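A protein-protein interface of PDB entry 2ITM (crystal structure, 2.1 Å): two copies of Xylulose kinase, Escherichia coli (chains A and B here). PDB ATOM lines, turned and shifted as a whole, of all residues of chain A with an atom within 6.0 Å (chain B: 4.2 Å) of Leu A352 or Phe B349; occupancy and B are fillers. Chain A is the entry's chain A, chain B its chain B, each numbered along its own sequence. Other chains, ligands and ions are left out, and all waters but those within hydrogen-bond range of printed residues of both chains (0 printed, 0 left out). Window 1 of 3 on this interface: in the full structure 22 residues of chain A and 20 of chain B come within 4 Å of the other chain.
Of the 12 printed residues of chain B, 8 touch a printed residue of chain A.
Hydrophobic or aromatic side chains of chain A that line the printed part of chain B: Val A348, Phe A349, Leu A352, His A356 and Leu A361.
Among the printed residues, no Asp or Glu carboxylate lies within 4 Å of a Lys or Arg side-chain nitrogen of the other chain.
N of Gly A347 is in hydrogen-bond range of O of Leu B352 (2.8 Å).
The backbone NH (N) of Phe A349 is in hydrogen-bond range of the backbone carbonyl oxygen (O) of Phe B349, at 3.1 Å.
The backbone carbonyl oxygen (O) of Leu A352 sits at hydrogen-bond distance from the backbone NH (N) of Gly B347.
NE1 of Trp B300 sits at hydrogen-bond distance from O of Thr A353.
The backbone NH (N) of His A354 lies close to the indole nitrogen (NE1) of Trp B300, 3.4 Å away.
Val B348 touches Val A348 (CG1 to CG1, 3.9 Å).
O of Phe B349 touches CG1 of Val A348, at 3.3 Å.
CG2 of Val A348 touches CD1 of Phe B350, 3.9 Å away.
O of Phe A349 touches CA of Val B348, 3.3 Å away.
Phe A349 touches Leu B352.
Leu A352 touches Lys B346.
CD1 of Leu A352 touches CD1 of Phe B349, at 3.8 Å.
CG2 of Thr A353 touches CG of Lys B346 (3.7 Å).
His A356 touches Leu B304 (O to CD1, 2.9 Å).
Leu A361 touches Leu B304 (CD2 to O, 3.6 Å).
The backbone carbonyl oxygen of Gly A351 is in hydrogen-bond range of a ring nitrogen (NE2) of His A356, at 3.4 Å.
The side-chain hydroxyl (OG1) of Thr A353 is in hydrogen-bond range of a ring nitrogen (NE2) of His A356 (3.4 Å).
The backbone NH (N) of Phe B350 lies within hydrogen-bond range of the backbone carbonyl oxygen (O) of Trp B328, at 2.8 Å.
Phe B349 touches three residues of chain A.
Of the printed residues of chain A, Leu B352 touches Gly A347 (2.8 Å) and Phe A349 (3.8 Å).
Of the printed residues of chain A, Lys B346 touches Leu A352 (3.0 Å) and Thr A353 (3.7 Å).
Printed residues of chain B within 4 Å of Leu A361: Leu B304 (3.6 Å).
Printed residues of chain B within 4 Å of His A354: Trp B300.
The nearest printed residue of chain B that does not touch Leu A352 is Leu B304 (4.02 Å).
The nearest residue of chain A that does not touch Phe B349 is Gly A347 (4.2 Å).
Gly A347 touches Leu B352, and with the chains exchanged Leu A352 touches Gly B347.
Val B348 touches its own counterpart, Val A348.
Val A348 touches Phe B349, and with the chains exchanged Phe A349 touches Val B348.
Val A348 touches Phe B350, but with the chains exchanged Phe A350 does not touch Val B348 (4.03 Å).
6 positions are printed for both chains.
Of the 17 pairs that touch across the chains among the printed residues, 8 have their exchanged pair printed and touching as well.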
ATOM      1  N   PRO A 326     -20.722  -8.311 -24.537  1.00  0.00           N
ATOM      2  CA  PRO A 326     -20.705  -6.928 -24.025  1.00  0.00           C
ATOM      3  C   PRO A 326     -21.644  -6.051 -24.830  1.00  0.00           C
ATOM      4  O   PRO A 326     -21.693  -6.166 -26.044  1.00  0.00           O
ATOM      5  CB  PRO A 326     -19.256  -6.504 -24.239  1.00  0.00           C
ATOM      6  CG  PRO A 326     -18.510  -7.762 -24.331  1.00  0.00           C
ATOM      7  CD  PRO A 326     -19.397  -8.729 -25.012  1.00  0.00           C
ATOM      8  N   VAL A 327     -22.395  -5.213 -24.132  1.00  0.00           N
ATOM      9  CA  VAL A 327     -22.884  -3.954 -24.655  1.00  0.00           C
ATOM     10  C   VAL A 327     -21.810  -2.909 -24.484  1.00  0.00           C
ATOM     11  O   VAL A 327     -21.122  -2.894 -23.483  1.00  0.00           O
ATOM     12  CB  VAL A 327     -24.098  -3.474 -23.861  1.00  0.00           C
ATOM     13  CG1 VAL A 327     -24.725  -2.305 -24.521  1.00  0.00           C
ATOM     14  CG2 VAL A 327     -25.086  -4.568 -23.707  1.00  0.00           C
ATOM     15  N   GLY A 347     -24.432  10.055 -25.843  1.00  0.00           N
ATOM     16  CA  GLY A 347     -24.062   8.671 -25.660  1.00  0.00           C
ATOM     17  C   GLY A 347     -24.552   7.763 -26.762  1.00  0.00           C
ATOM     18  O   GLY A 347     -25.560   8.024 -27.404  1.00  0.00           O
ATOM     19  N   VAL A 348     -23.824   6.679 -26.965  1.00  0.00           N
ATOM     20  CA  VAL A 348     -24.262   5.590 -27.816  1.00  0.00           C
ATOM     21  C   VAL A 348     -24.290   4.270 -27.058  1.00  0.00           C
ATOM     22  O   VAL A 348     -23.349   3.942 -26.361  1.00  0.00           O
ATOM     23  CB  VAL A 348     -23.384   5.462 -29.048  1.00  0.00           C
ATOM     24  CG1 VAL A 348     -23.970   4.483 -30.005  1.00  0.00           C
ATOM     25  CG2 VAL A 348     -23.195   6.805 -29.711  1.00  0.00           C
ATOM     26  N   PHE A 349     -25.387   3.533 -27.190  1.00  0.00           N
ATOM     27  CA  PHE A 349     -25.425   2.111 -26.853  1.00  0.00           C
ATOM     28  C   PHE A 349     -25.211   1.247 -28.090  1.00  0.00           C
ATOM     29  O   PHE A 349     -26.058   1.185 -28.964  1.00  0.00           O
ATOM     30  CB  PHE A 349     -26.752   1.733 -26.193  1.00  0.00           C
ATOM     31  CG  PHE A 349     -26.782   1.921 -24.725  1.00  0.00           C
ATOM     32  CD1 PHE A 349     -27.759   2.677 -24.131  1.00  0.00           C
ATOM     33  CD2 PHE A 349     -25.854   1.309 -23.922  1.00  0.00           C
ATOM     34  CE1 PHE A 349     -27.797   2.832 -22.762  1.00  0.00           C
ATOM     35  CE2 PHE A 349     -25.882   1.467 -22.572  1.00  0.00           C
ATOM     36  CZ  PHE A 349     -26.852   2.229 -21.989  1.00  0.00           C
ATOM     37  N   PHE A 350     -24.064   0.591 -28.136  1.00  0.00           N
ATOM     38  CA  PHE A 350     -23.640  -0.197 -29.275  1.00  0.00           C
ATOM     39  C   PHE A 350     -23.617  -1.695 -28.986  1.00  0.00           C
ATOM     40  O   PHE A 350     -23.041  -2.132 -28.026  1.00  0.00           O
ATOM     41  CB  PHE A 350     -22.259   0.256 -29.738  1.00  0.00           C
ATOM     42  CG  PHE A 350     -21.774  -0.453 -30.950  1.00  0.00           C
ATOM     43  CD1 PHE A 350     -22.163  -0.044 -32.205  1.00  0.00           C
ATOM     44  CD2 PHE A 350     -20.946  -1.536 -30.837  1.00  0.00           C
ATOM     45  CE1 PHE A 350     -21.733  -0.695 -33.307  1.00  0.00           C
ATOM     46  CE2 PHE A 350     -20.516  -2.193 -31.940  1.00  0.00           C
ATOM     47  CZ  PHE A 350     -20.911  -1.772 -33.180  1.00  0.00           C
ATOM     48  N   GLY A 351     -24.232  -2.468 -29.863  1.00  0.00           N
ATOM     49  CA  GLY A 351     -24.083  -3.920 -29.844  1.00  0.00           C
ATOM     50  C   GLY A 351     -25.093  -4.634 -28.987  1.00  0.00           C
ATOM     51  O   GLY A 351     -24.770  -5.624 -28.360  1.00  0.00           O
ATOM     52  N   LEU A 352     -26.311  -4.143 -28.931  1.00  0.00           N
ATOM     53  CA  LEU A 352     -27.362  -4.737 -28.148  1.00  0.00           C
ATOM     54  C   LEU A 352     -27.975  -5.960 -28.819  1.00  0.00           C
ATOM     55  O   LEU A 352     -28.234  -5.952 -29.993  1.00  0.00           O
ATOM     56  CB  LEU A 352     -28.460  -3.719 -27.852  1.00  0.00           C
ATOM     57  CG  LEU A 352     -28.084  -2.303 -27.396  1.00  0.00           C
ATOM     58  CD1 LEU A 352     -29.067  -1.310 -27.901  1.00  0.00           C
ATOM     59  CD2 LEU A 352     -27.976  -2.214 -25.895  1.00  0.00           C
ATOM     60  N   THR A 353     -28.200  -7.007 -28.029  1.00  0.00           N
ATOM     61  CA  THR A 353     -28.792  -8.256 -28.495  1.00  0.00           C
ATOM     62  C   THR A 353     -29.892  -8.739 -27.568  1.00  0.00           C
ATOM     63  O   THR A 353     -30.117  -8.172 -26.518  1.00  0.00           O
ATOM     64  CB  THR A 353     -27.737  -9.350 -28.589  1.00  0.00           C
ATOM     65  OG1 THR A 353     -27.315  -9.715 -27.276  1.00  0.00           O
ATOM     66  CG2 THR A 353     -26.484  -8.835 -29.224  1.00  0.00           C
ATOM     67  N   HIS A 354     -30.558  -9.814 -27.974  1.00  0.00           N
ATOM     68  CA  HIS A 354     -31.567 -10.484 -27.168  1.00  0.00           C
ATOM     69  C   HIS A 354     -31.135 -10.738 -25.727  1.00  0.00           C
ATOM     70  O   HIS A 354     -31.977 -10.924 -24.849  1.00  0.00           O
ATOM     71  CB  HIS A 354     -31.980 -11.798 -27.828  1.00  0.00           C
ATOM     72  CG  HIS A 354     -30.922 -12.859 -27.781  1.00  0.00           C
ATOM     73  ND1 HIS A 354     -29.809 -12.838 -28.590  1.00  0.00           N
ATOM     74  CD2 HIS A 354     -30.806 -13.969 -27.015  1.00  0.00           C
ATOM     75  CE1 HIS A 354     -29.056 -13.888 -28.332  1.00  0.00           C
ATOM     76  NE2 HIS A 354     -29.639 -14.593 -27.382  1.00  0.00           N
ATOM     77  N   HIS A 356     -29.696  -8.909 -23.614  1.00  0.00           N
ATOM     78  CA  HIS A 356     -29.445  -7.723 -22.823  1.00  0.00           C
ATOM     79  C   HIS A 356     -30.724  -7.219 -22.153  1.00  0.00           C
ATOM     80  O   HIS A 356     -31.724  -6.995 -22.805  1.00  0.00           O
ATOM     81  CB  HIS A 356     -28.828  -6.611 -23.669  1.00  0.00           C
ATOM     82  CG  HIS A 356     -27.498  -6.960 -24.255  1.00  0.00           C
ATOM     83  ND1 HIS A 356     -26.490  -7.534 -23.518  1.00  0.00           N
ATOM     84  CD2 HIS A 356     -27.010  -6.807 -25.504  1.00  0.00           C
ATOM     85  CE1 HIS A 356     -25.439  -7.727 -24.290  1.00  0.00           C
ATOM     86  NE2 HIS A 356     -25.729  -7.291 -25.500  1.00  0.00           N
ATOM     87  N   LEU A 361     -27.261  -3.271 -19.330  1.00  0.00           N
ATOM     88  CA  LEU A 361     -27.207  -1.873 -19.701  1.00  0.00           C
ATOM     89  C   LEU A 361     -26.493  -1.066 -18.638  1.00  0.00           C
ATOM     90  O   LEU A 361     -25.669  -0.223 -18.934  1.00  0.00           O
ATOM     91  CB  LEU A 361     -28.610  -1.338 -19.927  1.00  0.00           C
ATOM     92  CG  LEU A 361     -28.980  -1.253 -21.397  1.00  0.00           C
ATOM     93  CD1 LEU A 361     -28.381  -2.386 -22.153  1.00  0.00           C
ATOM     94  CD2 LEU A 361     -30.479  -1.166 -21.622  1.00  0.00           C
ATOM     95  N   TRP B 300     -38.529  -7.556 -27.978  1.00  0.00           N
ATOM     96  CA  TRP B 300     -37.166  -7.467 -27.496  1.00  0.00           C
ATOM     97  C   TRP B 300     -36.916  -6.133 -26.824  1.00  0.00           C
ATOM     98  O   TRP B 300     -36.332  -6.059 -25.756  1.00  0.00           O
ATOM     99  CB  TRP B 300     -36.192  -7.670 -28.638  1.00  0.00           C
ATOM    100  CG  TRP B 300     -34.785  -7.423 -28.266  1.00  0.00           C
ATOM    101  CD1 TRP B 300     -34.140  -7.855 -27.151  1.00  0.00           C
ATOM    102  CD2 TRP B 300     -33.833  -6.684 -29.018  1.00  0.00           C
ATOM    103  NE1 TRP B 300     -32.837  -7.428 -27.166  1.00  0.00           N
ATOM    104  CE2 TRP B 300     -32.626  -6.711 -28.310  1.00  0.00           C
ATOM    105  CE3 TRP B 300     -33.877  -6.009 -30.234  1.00  0.00           C
ATOM    106  CZ2 TRP B 300     -31.488  -6.084 -28.767  1.00  0.00           C
ATOM    107  CZ3 TRP B 300     -32.750  -5.393 -30.685  1.00  0.00           C
ATOM    108  CH2 TRP B 300     -31.569  -5.433 -29.958  1.00  0.00           C
ATOM    109  N   LEU B 304     -35.384  -5.269 -23.211  1.00  0.00           N
ATOM    110  CA  LEU B 304     -34.238  -4.382 -23.190  1.00  0.00           C
ATOM    111  C   LEU B 304     -34.461  -3.179 -22.303  1.00  0.00           C
ATOM    112  O   LEU B 304     -33.611  -2.855 -21.495  1.00  0.00           O
ATOM    113  CB  LEU B 304     -33.902  -3.915 -24.598  1.00  0.00           C
ATOM    114  CG  LEU B 304     -32.467  -3.476 -24.840  1.00  0.00           C
ATOM    115  CD1 LEU B 304     -31.532  -4.390 -24.127  1.00  0.00           C
ATOM    116  CD2 LEU B 304     -32.164  -3.471 -26.313  1.00  0.00           C
ATOM    117  N   TRP B 328     -32.115   8.062 -31.844  1.00  0.00           N
ATOM    118  CA  TRP B 328     -32.296   7.139 -32.934  1.00  0.00           C
ATOM    119  C   TRP B 328     -32.071   5.700 -32.506  1.00  0.00           C
ATOM    120  O   TRP B 328     -31.043   5.361 -31.942  1.00  0.00           O
ATOM    121  CB  TRP B 328     -31.381   7.539 -34.086  1.00  0.00           C
ATOM    122  CG  TRP B 328     -31.345   9.025 -34.256  1.00  0.00           C
ATOM    123  CD1 TRP B 328     -30.691   9.929 -33.471  1.00  0.00           C
ATOM    124  CD2 TRP B 328     -32.037   9.781 -35.229  1.00  0.00           C
ATOM    125  NE1 TRP B 328     -30.921  11.204 -33.912  1.00  0.00           N
ATOM    126  CE2 TRP B 328     -31.747  11.137 -34.998  1.00  0.00           C
ATOM    127  CE3 TRP B 328     -32.865   9.453 -36.290  1.00  0.00           C
ATOM    128  CZ2 TRP B 328     -32.250  12.143 -35.786  1.00  0.00           C
ATOM    129  CZ3 TRP B 328     -33.355  10.440 -37.055  1.00  0.00           C
ATOM    130  CH2 TRP B 328     -33.054  11.774 -36.807  1.00  0.00           C
ATOM    131  N   PHE B 329     -33.060   4.859 -32.763  1.00  0.00           N
ATOM    132  CA  PHE B 329     -32.932   3.432 -32.561  1.00  0.00           C
ATOM    133  C   PHE B 329     -32.736   2.715 -33.874  1.00  0.00           C
ATOM    134  O   PHE B 329     -33.559   2.815 -34.770  1.00  0.00           O
ATOM    135  CB  PHE B 329     -34.160   2.886 -31.849  1.00  0.00           C
ATOM    136  CG  PHE B 329     -34.169   1.394 -31.714  1.00  0.00           C
ATOM    137  CD1 PHE B 329     -33.216   0.749 -30.957  1.00  0.00           C
ATOM    138  CD2 PHE B 329     -35.140   0.640 -32.330  1.00  0.00           C
ATOM    139  CE1 PHE B 329     -33.222  -0.611 -30.834  1.00  0.00           C
ATOM    140  CE2 PHE B 329     -35.154  -0.721 -32.213  1.00  0.00           C
ATOM    141  CZ  PHE B 329     -34.195  -1.351 -31.468  1.00  0.00           C
ATOM    142  N   LYS B 346     -30.301  -7.413 -33.446  1.00  0.00           N
ATOM    143  CA  LYS B 346     -29.511  -6.532 -32.615  1.00  0.00           C
ATOM    144  C   LYS B 346     -29.920  -5.082 -32.784  1.00  0.00           C
ATOM    145  O   LYS B 346     -30.839  -4.815 -33.498  1.00  0.00           O
ATOM    146  CB  LYS B 346     -28.063  -6.701 -32.957  1.00  0.00           C
ATOM    147  CG  LYS B 346     -27.590  -8.038 -32.630  1.00  0.00           C
ATOM    148  CD  LYS B 346     -26.436  -8.478 -33.475  1.00  0.00           C
ATOM    149  CE  LYS B 346     -25.815  -9.731 -32.870  1.00  0.00           C
ATOM    150  NZ  LYS B 346     -26.751 -10.879 -32.666  1.00  0.00           N
ATOM    151  N   GLY B 347     -29.229  -4.168 -32.122  1.00  0.00           N
ATOM    152  CA  GLY B 347     -29.555  -2.755 -32.205  1.00  0.00           C
ATOM    153  C   GLY B 347     -28.614  -1.718 -31.612  1.00  0.00           C
ATOM    154  O   GLY B 347     -27.707  -2.070 -30.900  1.00  0.00           O
ATOM    155  N   VAL B 348     -28.875  -0.452 -31.931  1.00  0.00           N
ATOM    156  CA  VAL B 348     -28.122   0.698 -31.472  1.00  0.00           C
ATOM    157  C   VAL B 348     -29.082   1.820 -31.077  1.00  0.00           C
ATOM    158  O   VAL B 348     -30.025   2.113 -31.795  1.00  0.00           O
ATOM    159  CB  VAL B 348     -27.158   1.218 -32.589  1.00  0.00           C
ATOM    160  CG1 VAL B 348     -26.507   2.506 -32.184  1.00  0.00           C
ATOM    161  CG2 VAL B 348     -26.115   0.183 -32.957  1.00  0.00           C
ATOM    162  N   PHE B 349     -28.833   2.433 -29.927  1.00  0.00           N
ATOM    163  CA  PHE B 349     -29.328   3.772 -29.634  1.00  0.00           C
ATOM    164  C   PHE B 349     -28.265   4.830 -29.883  1.00  0.00           C
ATOM    165  O   PHE B 349     -27.162   4.735 -29.374  1.00  0.00           O
ATOM    166  CB  PHE B 349     -29.763   3.883 -28.181  1.00  0.00           C
ATOM    167  CG  PHE B 349     -30.983   3.112 -27.842  1.00  0.00           C
ATOM    168  CD1 PHE B 349     -30.894   1.969 -27.101  1.00  0.00           C
ATOM    169  CD2 PHE B 349     -32.225   3.547 -28.229  1.00  0.00           C
ATOM    170  CE1 PHE B 349     -32.018   1.269 -26.769  1.00  0.00           C
ATOM    171  CE2 PHE B 349     -33.341   2.847 -27.897  1.00  0.00           C
ATOM    172  CZ  PHE B 349     -33.238   1.712 -27.171  1.00  0.00           C
ATOM    173  N   PHE B 350     -28.616   5.845 -30.655  1.00  0.00           N
ATOM    174  CA  PHE B 350     -27.684   6.896 -31.026  1.00  0.00           C
ATOM    175  C   PHE B 350     -28.278   8.254 -30.686  1.00  0.00           C
ATOM    176  O   PHE B 350     -29.344   8.594 -31.135  1.00  0.00           O
ATOM    177  CB  PHE B 350     -27.359   6.795 -32.495  1.00  0.00           C
ATOM    178  CG  PHE B 350     -26.196   7.653 -32.940  1.00  0.00           C
ATOM    179  CD1 PHE B 350     -24.951   7.111 -33.170  1.00  0.00           C
ATOM    180  CD2 PHE B 350     -26.371   8.995 -33.157  1.00  0.00           C
ATOM    181  CE1 PHE B 350     -23.910   7.895 -33.589  1.00  0.00           C
ATOM    182  CE2 PHE B 350     -25.327   9.779 -33.581  1.00  0.00           C
ATOM    183  CZ  PHE B 350     -24.098   9.227 -33.792  1.00  0.00           C
ATOM    184  N   LEU B 352     -28.116   9.634 -27.260  1.00  0.00           N
ATOM    185  CA  LEU B 352     -28.645   9.614 -25.923  1.00  0.00           C
ATOM    186  C   LEU B 352     -28.108  10.801 -25.148  1.00  0.00           C
ATOM    187  O   LEU B 352     -26.916  11.059 -25.139  1.00  0.00           O
ATOM    188  CB  LEU B 352     -28.291   8.310 -25.229  1.00  0.00           C
ATOM    189  CG  LEU B 352     -29.393   7.288 -24.967  1.00  0.00           C
ATOM    190  CD1 LEU B 352     -30.751   7.723 -25.410  1.00  0.00           C
ATOM    191  CD2 LEU B 352     -29.042   5.967 -25.522  1.00  0.00           C
ATOM    192  N   LEU B 361     -36.899   6.405 -24.607  1.00  0.00           N
ATOM    193  CA  LEU B 361     -36.270   5.260 -25.203  1.00  0.00           C
ATOM    194  C   LEU B 361     -37.297   4.442 -25.969  1.00  0.00           C
ATOM    195  O   LEU B 361     -37.014   3.903 -27.025  1.00  0.00           O
ATOM    196  CB  LEU B 361     -35.606   4.426 -24.115  1.00  0.00           C
ATOM    197  CG  LEU B 361     -34.148   4.010 -24.271  1.00  0.00           C
ATOM    198  CD1 LEU B 361     -33.233   5.184 -24.385  1.00  0.00           C
ATOM    199  CD2 LEU B 361     -33.763   3.142 -23.114  1.00  0.00           C
ATOM    200  N   VAL B 365     -37.680   3.475 -30.021  1.00  0.00           N
ATOM    201  CA  VAL B 365     -37.915   2.147 -30.553  1.00  0.00           C
ATOM    202  C   VAL B 365     -39.063   2.108 -31.559  1.00  0.00           C
ATOM    203  O   VAL B 365     -38.930   1.523 -32.608  1.00  0.00           O
ATOM    204  CB  VAL B 365     -38.163   1.142 -29.433  1.00  0.00           C
ATOM    205  CG1 VAL B 365     -38.418  -0.226 -29.990  1.00  0.00           C
ATOM    206  CG2 VAL B 365     -37.001   1.125 -28.486  1.00  0.00           C
